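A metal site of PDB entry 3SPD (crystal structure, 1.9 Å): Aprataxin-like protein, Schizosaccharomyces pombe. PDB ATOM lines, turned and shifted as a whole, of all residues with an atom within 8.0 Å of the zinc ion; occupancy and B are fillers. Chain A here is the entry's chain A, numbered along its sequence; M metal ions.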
ATOM      1  N   TYR A 138      32.426  24.917 -12.448  1.00  0.00           N
ATOM      2  CA  TYR A 138      31.008  24.681 -12.726  1.00  0.00           C
ATOM      3  C   TYR A 138      30.164  25.047 -11.526  1.00  0.00           C
ATOM      4  O   TYR A 138      29.162  25.753 -11.643  1.00  0.00           O
ATOM      5  CB  TYR A 138      30.797  23.209 -13.079  1.00  0.00           C
ATOM      6  CG  TYR A 138      29.367  22.857 -13.368  1.00  0.00           C
ATOM      7  CD1 TYR A 138      28.781  23.207 -14.584  1.00  0.00           C
ATOM      8  CD2 TYR A 138      28.590  22.172 -12.442  1.00  0.00           C
ATOM      9  CE1 TYR A 138      27.467  22.879 -14.867  1.00  0.00           C
ATOM     10  CE2 TYR A 138      27.289  21.825 -12.725  1.00  0.00           C
ATOM     11  CZ  TYR A 138      26.729  22.189 -13.919  1.00  0.00           C
ATOM     12  OH  TYR A 138      25.405  21.849 -14.186  1.00  0.00           O
ATOM     13  N   LYS A 171      25.608  18.131 -10.519  1.00  0.00           N
ATOM     14  CA  LYS A 171      24.307  17.922 -11.143  1.00  0.00           C
ATOM     15  C   LYS A 171      24.161  18.876 -12.313  1.00  0.00           C
ATOM     16  O   LYS A 171      24.570  20.025 -12.245  1.00  0.00           O
ATOM     17  CB  LYS A 171      23.169  18.138 -10.132  1.00  0.00           C
ATOM     18  CG  LYS A 171      23.228  19.475  -9.430  1.00  0.00           C
ATOM     19  CD  LYS A 171      22.086  19.656  -8.422  1.00  0.00           C
ATOM     20  CE  LYS A 171      22.196  21.035  -7.743  1.00  0.00           C
ATOM     21  NZ  LYS A 171      21.264  21.221  -6.588  1.00  0.00           N
ATOM     22  N   CYS A 172      23.604  18.359 -13.413  1.00  0.00           N
ATOM     23  CA  CYS A 172      23.326  19.185 -14.572  1.00  0.00           C
ATOM     24  C   CYS A 172      22.334  20.286 -14.200  1.00  0.00           C
ATOM     25  O   CYS A 172      21.312  20.011 -13.570  1.00  0.00           O
ATOM     26  CB  CYS A 172      22.750  18.333 -15.691  1.00  0.00           C
ATOM     27  SG  CYS A 172      22.155  19.265 -17.127  1.00  0.00           S
ATOM     28  N   TRP A 173      22.630  21.518 -14.569  1.00  0.00           N
ATOM     29  CA  TRP A 173      21.734  22.625 -14.228  1.00  0.00           C
ATOM     30  C   TRP A 173      20.401  22.534 -14.979  1.00  0.00           C
ATOM     31  O   TRP A 173      19.398  23.056 -14.527  1.00  0.00           O
ATOM     32  CB  TRP A 173      22.394  23.966 -14.548  1.00  0.00           C
ATOM     33  CG  TRP A 173      22.638  24.144 -16.000  1.00  0.00           C
ATOM     34  CD1 TRP A 173      23.778  23.817 -16.678  1.00  0.00           C
ATOM     35  CD2 TRP A 173      21.736  24.667 -16.967  1.00  0.00           C
ATOM     36  NE1 TRP A 173      23.637  24.112 -18.014  1.00  0.00           N
ATOM     37  CE2 TRP A 173      22.389  24.633 -18.214  1.00  0.00           C
ATOM     38  CE3 TRP A 173      20.419  25.165 -16.897  1.00  0.00           C
ATOM     39  CZ2 TRP A 173      21.781  25.080 -19.379  1.00  0.00           C
ATOM     40  CZ3 TRP A 173      19.828  25.607 -18.060  1.00  0.00           C
ATOM     41  CH2 TRP A 173      20.508  25.565 -19.289  1.00  0.00           C
ATOM     42  N   ARG A 174      20.395  21.887 -16.132  1.00  0.00           N
ATOM     43  CA  ARG A 174      19.207  21.910 -16.986  1.00  0.00           C
ATOM     44  C   ARG A 174      18.206  20.788 -16.699  1.00  0.00           C
ATOM     45  O   ARG A 174      16.994  21.029 -16.684  1.00  0.00           O
ATOM     46  CB  ARG A 174      19.597  21.930 -18.467  1.00  0.00           C
ATOM     47  CG  ARG A 174      18.416  22.082 -19.433  1.00  0.00           C
ATOM     48  CD  ARG A 174      18.859  22.443 -20.845  1.00  0.00           C
ATOM     49  NE  ARG A 174      17.725  22.790 -21.702  1.00  0.00           N
ATOM     50  CZ  ARG A 174      17.304  22.084 -22.737  1.00  0.00           C
ATOM     51  NH1 ARG A 174      17.936  20.963 -23.087  1.00  0.00           N
ATOM     52  NH2 ARG A 174      16.258  22.497 -23.437  1.00  0.00           N
ATOM     53  N   CYS A 175      18.695  19.572 -16.476  1.00  0.00           N
ATOM     54  CA  CYS A 175      17.809  18.416 -16.357  1.00  0.00           C
ATOM     55  C   CYS A 175      17.932  17.696 -15.019  1.00  0.00           C
ATOM     56  O   CYS A 175      17.156  16.792 -14.726  1.00  0.00           O
ATOM     57  CB  CYS A 175      18.061  17.414 -17.484  1.00  0.00           C
ATOM     58  SG  CYS A 175      19.424  16.299 -17.093  1.00  0.00           S
ATOM     59  N   GLY A 176      18.915  18.092 -14.213  1.00  0.00           N
ATOM     60  CA  GLY A 176      19.042  17.565 -12.859  1.00  0.00           C
ATOM     61  C   GLY A 176      19.834  16.274 -12.710  1.00  0.00           C
ATOM     62  O   GLY A 176      20.126  15.851 -11.589  1.00  0.00           O
ATOM     63  N   GLU A 177      20.177  15.644 -13.832  1.00  0.00           N
ATOM     64  CA  GLU A 177      21.005  14.435 -13.819  1.00  0.00           C
ATOM     65  C   GLU A 177      22.273  14.645 -13.000  1.00  0.00           C
ATOM     66  O   GLU A 177      22.883  15.712 -13.040  1.00  0.00           O
ATOM     67  CB  GLU A 177      21.361  13.992 -15.248  1.00  0.00           C
ATOM     68  CG  GLU A 177      22.131  12.680 -15.299  1.00  0.00           C
ATOM     69  CD  GLU A 177      22.394  12.193 -16.715  1.00  0.00           C
ATOM     70  OE1 GLU A 177      21.740  12.676 -17.671  1.00  0.00           O
ATOM     71  OE2 GLU A 177      23.260  11.301 -16.875  1.00  0.00           O
ATOM     72  N   THR A 178      22.649  13.614 -12.235  1.00  0.00           N
ATOM     73  CA  THR A 178      23.809  13.705 -11.348  1.00  0.00           C
ATOM     74  C   THR A 178      24.993  12.923 -11.912  1.00  0.00           C
ATOM     75  O   THR A 178      24.826  11.996 -12.709  1.00  0.00           O
ATOM     76  CB  THR A 178      23.478  13.182  -9.934  1.00  0.00           C
ATOM     77  OG1 THR A 178      23.040  11.819 -10.018  1.00  0.00           O
ATOM     78  CG2 THR A 178      22.367  14.032  -9.319  1.00  0.00           C
ATOM     79  N   PHE A 179      26.194  13.328 -11.503  1.00  0.00           N
ATOM     80  CA  PHE A 179      27.425  12.790 -12.080  1.00  0.00           C
ATOM     81  C   PHE A 179      28.502  12.518 -11.037  1.00  0.00           C
ATOM     82  O   PHE A 179      29.669  12.311 -11.383  1.00  0.00           O
ATOM     83  CB  PHE A 179      27.955  13.765 -13.119  1.00  0.00           C
ATOM     84  CG  PHE A 179      27.097  13.866 -14.343  1.00  0.00           C
ATOM     85  CD1 PHE A 179      27.273  12.973 -15.384  1.00  0.00           C
ATOM     86  CD2 PHE A 179      26.120  14.846 -14.455  1.00  0.00           C
ATOM     87  CE1 PHE A 179      26.487  13.054 -16.513  1.00  0.00           C
ATOM     88  CE2 PHE A 179      25.326  14.922 -15.580  1.00  0.00           C
ATOM     89  CZ  PHE A 179      25.512  14.026 -16.604  1.00  0.00           C
ATOM     90  N   LEU A 186      30.138  15.036 -16.940  1.00  0.00           N
ATOM     91  CA  LEU A 186      29.277  16.220 -16.925  1.00  0.00           C
ATOM     92  C   LEU A 186      29.553  17.077 -18.160  1.00  0.00           C
ATOM     93  O   LEU A 186      28.622  17.468 -18.861  1.00  0.00           O
ATOM     94  CB  LEU A 186      29.510  17.058 -15.665  1.00  0.00           C
ATOM     95  CG  LEU A 186      28.795  18.418 -15.650  1.00  0.00           C
ATOM     96  CD1 LEU A 186      27.296  18.234 -15.509  1.00  0.00           C
ATOM     97  CD2 LEU A 186      29.325  19.286 -14.502  1.00  0.00           C
ATOM     98  N   HIS A 189      27.968  15.789 -21.247  1.00  0.00           N
ATOM     99  CA  HIS A 189      26.538  15.953 -21.127  1.00  0.00           C
ATOM    100  C   HIS A 189      26.111  17.409 -21.337  1.00  0.00           C
ATOM    101  O   HIS A 189      25.050  17.653 -21.891  1.00  0.00           O
ATOM    102  CB  HIS A 189      26.087  15.459 -19.766  1.00  0.00           C
ATOM    103  CG  HIS A 189      24.622  15.639 -19.517  1.00  0.00           C
ATOM    104  ND1 HIS A 189      23.680  14.735 -19.970  1.00  0.00           N
ATOM    105  CD2 HIS A 189      23.940  16.592 -18.859  1.00  0.00           C
ATOM    106  CE1 HIS A 189      22.479  15.147 -19.594  1.00  0.00           C
ATOM    107  NE2 HIS A 189      22.614  16.273 -18.923  1.00  0.00           N
ATOM    108  N   LEU A 190      26.931  18.364 -20.910  1.00  0.00           N
ATOM    109  CA  LEU A 190      26.594  19.777 -21.121  1.00  0.00           C
ATOM    110  C   LEU A 190      26.582  20.102 -22.598  1.00  0.00           C
ATOM    111  O   LEU A 190      25.754  20.875 -23.078  1.00  0.00           O
ATOM    112  CB  LEU A 190      27.573  20.692 -20.372  1.00  0.00           C
ATOM    113  CG  LEU A 190      27.413  20.645 -18.844  1.00  0.00           C
ATOM    114  CD1 LEU A 190      28.589  21.318 -18.178  1.00  0.00           C
ATOM    115  CD2 LEU A 190      26.103  21.322 -18.408  1.00  0.00           C
ATOM    116  N   GLU A 192      25.800  17.913 -25.001  1.00  0.00           N
ATOM    117  CA  GLU A 192      24.522  17.368 -25.456  1.00  0.00           C
ATOM    118  C   GLU A 192      23.352  18.280 -25.114  1.00  0.00           C
ATOM    119  O   GLU A 192      22.458  18.508 -25.945  1.00  0.00           O
ATOM    120  CB  GLU A 192      24.290  15.967 -24.860  1.00  0.00           C
ATOM    121  CG  GLU A 192      25.406  14.998 -25.202  1.00  0.00           C
ATOM    122  CD  GLU A 192      25.206  13.626 -24.585  1.00  0.00           C
ATOM    123  OE1 GLU A 192      24.559  13.526 -23.516  1.00  0.00           O
ATOM    124  OE2 GLU A 192      25.710  12.641 -25.178  1.00  0.00           O
ATOM    125  N   GLU A 193      23.348  18.814 -23.891  1.00  0.00           N
ATOM    126  CA  GLU A 193      22.259  19.659 -23.443  1.00  0.00           C
ATOM    127  C   GLU A 193      22.201  20.936 -24.263  1.00  0.00           C
ATOM    128  O   GLU A 193      21.120  21.446 -24.552  1.00  0.00           O
ATOM    129  CB  GLU A 193      22.411  20.031 -21.974  1.00  0.00           C
ATOM    130  CG  GLU A 193      21.999  18.936 -21.001  1.00  0.00           C
ATOM    131  CD  GLU A 193      20.490  18.814 -20.855  1.00  0.00           C
ATOM    132  OE1 GLU A 193      19.747  19.214 -21.783  1.00  0.00           O
ATOM    133  OE2 GLU A 193      20.044  18.325 -19.813  1.00  0.00           O
ATOM    134  N   TYR A 194      23.367  21.463 -24.623  1.00  0.00           N
ATOM    135  CA  TYR A 194      23.398  22.654 -25.450  1.00  0.00           C
ATOM    136  C   TYR A 194      22.837  22.331 -26.834  1.00  0.00           C
ATOM    137  O   TYR A 194      21.984  23.052 -27.353  1.00  0.00           O
ATOM    138  CB  TYR A 194      24.808  23.251 -25.591  1.00  0.00           C
ATOM    139  CG  TYR A 194      24.815  24.362 -26.616  1.00  0.00           C
ATOM    140  CD1 TYR A 194      24.295  25.617 -26.311  1.00  0.00           C
ATOM    141  CD2 TYR A 194      25.277  24.150 -27.907  1.00  0.00           C
ATOM    142  CE1 TYR A 194      24.258  26.625 -27.244  1.00  0.00           C
ATOM    143  CE2 TYR A 194      25.246  25.155 -28.856  1.00  0.00           C
ATOM    144  CZ  TYR A 194      24.737  26.393 -28.524  1.00  0.00           C
ATOM    145  OH  TYR A 194      24.708  27.406 -29.461  1.00  0.00           O
ATOM    146  N   ASP A 196      20.803  20.114 -27.680  1.00  0.00           N
ATOM    147  CA  ASP A 196      19.366  19.932 -27.540  1.00  0.00           C
ATOM    148  C   ASP A 196      18.632  21.272 -27.434  1.00  0.00           C
ATOM    149  O   ASP A 196      17.649  21.502 -28.131  1.00  0.00           O
ATOM    150  CB  ASP A 196      19.060  19.078 -26.310  1.00  0.00           C
ATOM    151  CG  ASP A 196      19.319  17.603 -26.542  1.00  0.00           C
ATOM    152  OD1 ASP A 196      19.748  17.250 -27.660  1.00  0.00           O
ATOM    153  OD2 ASP A 196      19.095  16.810 -25.609  1.00  0.00           O
HETATM  154 ZN    ZN M   1      21.076  17.541 -18.237  1.00  0.00          ZN
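OE1 of Glu 193 is in salt-bridge range of NH1 of Arg 174 (2.8 Å). The side-chain sulfur (SG) of Cys 172 sits close to the backbone NH (N) of Arg 174, at 3.3 Å. The backbone carbonyl oxygen of Glu 177 sits at hydrogen-bond distance from the backbone NH of Cys 172 (2.8 Å). The backbone NH of Glu 177 lies close to the side-chain sulfur of Cys 175, 3.4 Å away.
Four residues have an atom within 4 Å of the zinc ion: Cys 172, Cys 175, His 189 and Glu 193. Along chain A the residues within 4 Å of the zinc ion span positions 172 to 193.
The zinc ion is bound by the side-chain carboxylate (OE2) of Glu 193, at 2.0 Å. A ring nitrogen (NE2) of His 189 is bound to the zinc ion (2.1 Å). The side-chain sulfur (SG) of Cys 172 is bound to the zinc ion (2.3 Å). The side-chain sulfur (SG) of Cys 175 binds the zinc ion (2.4 Å).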
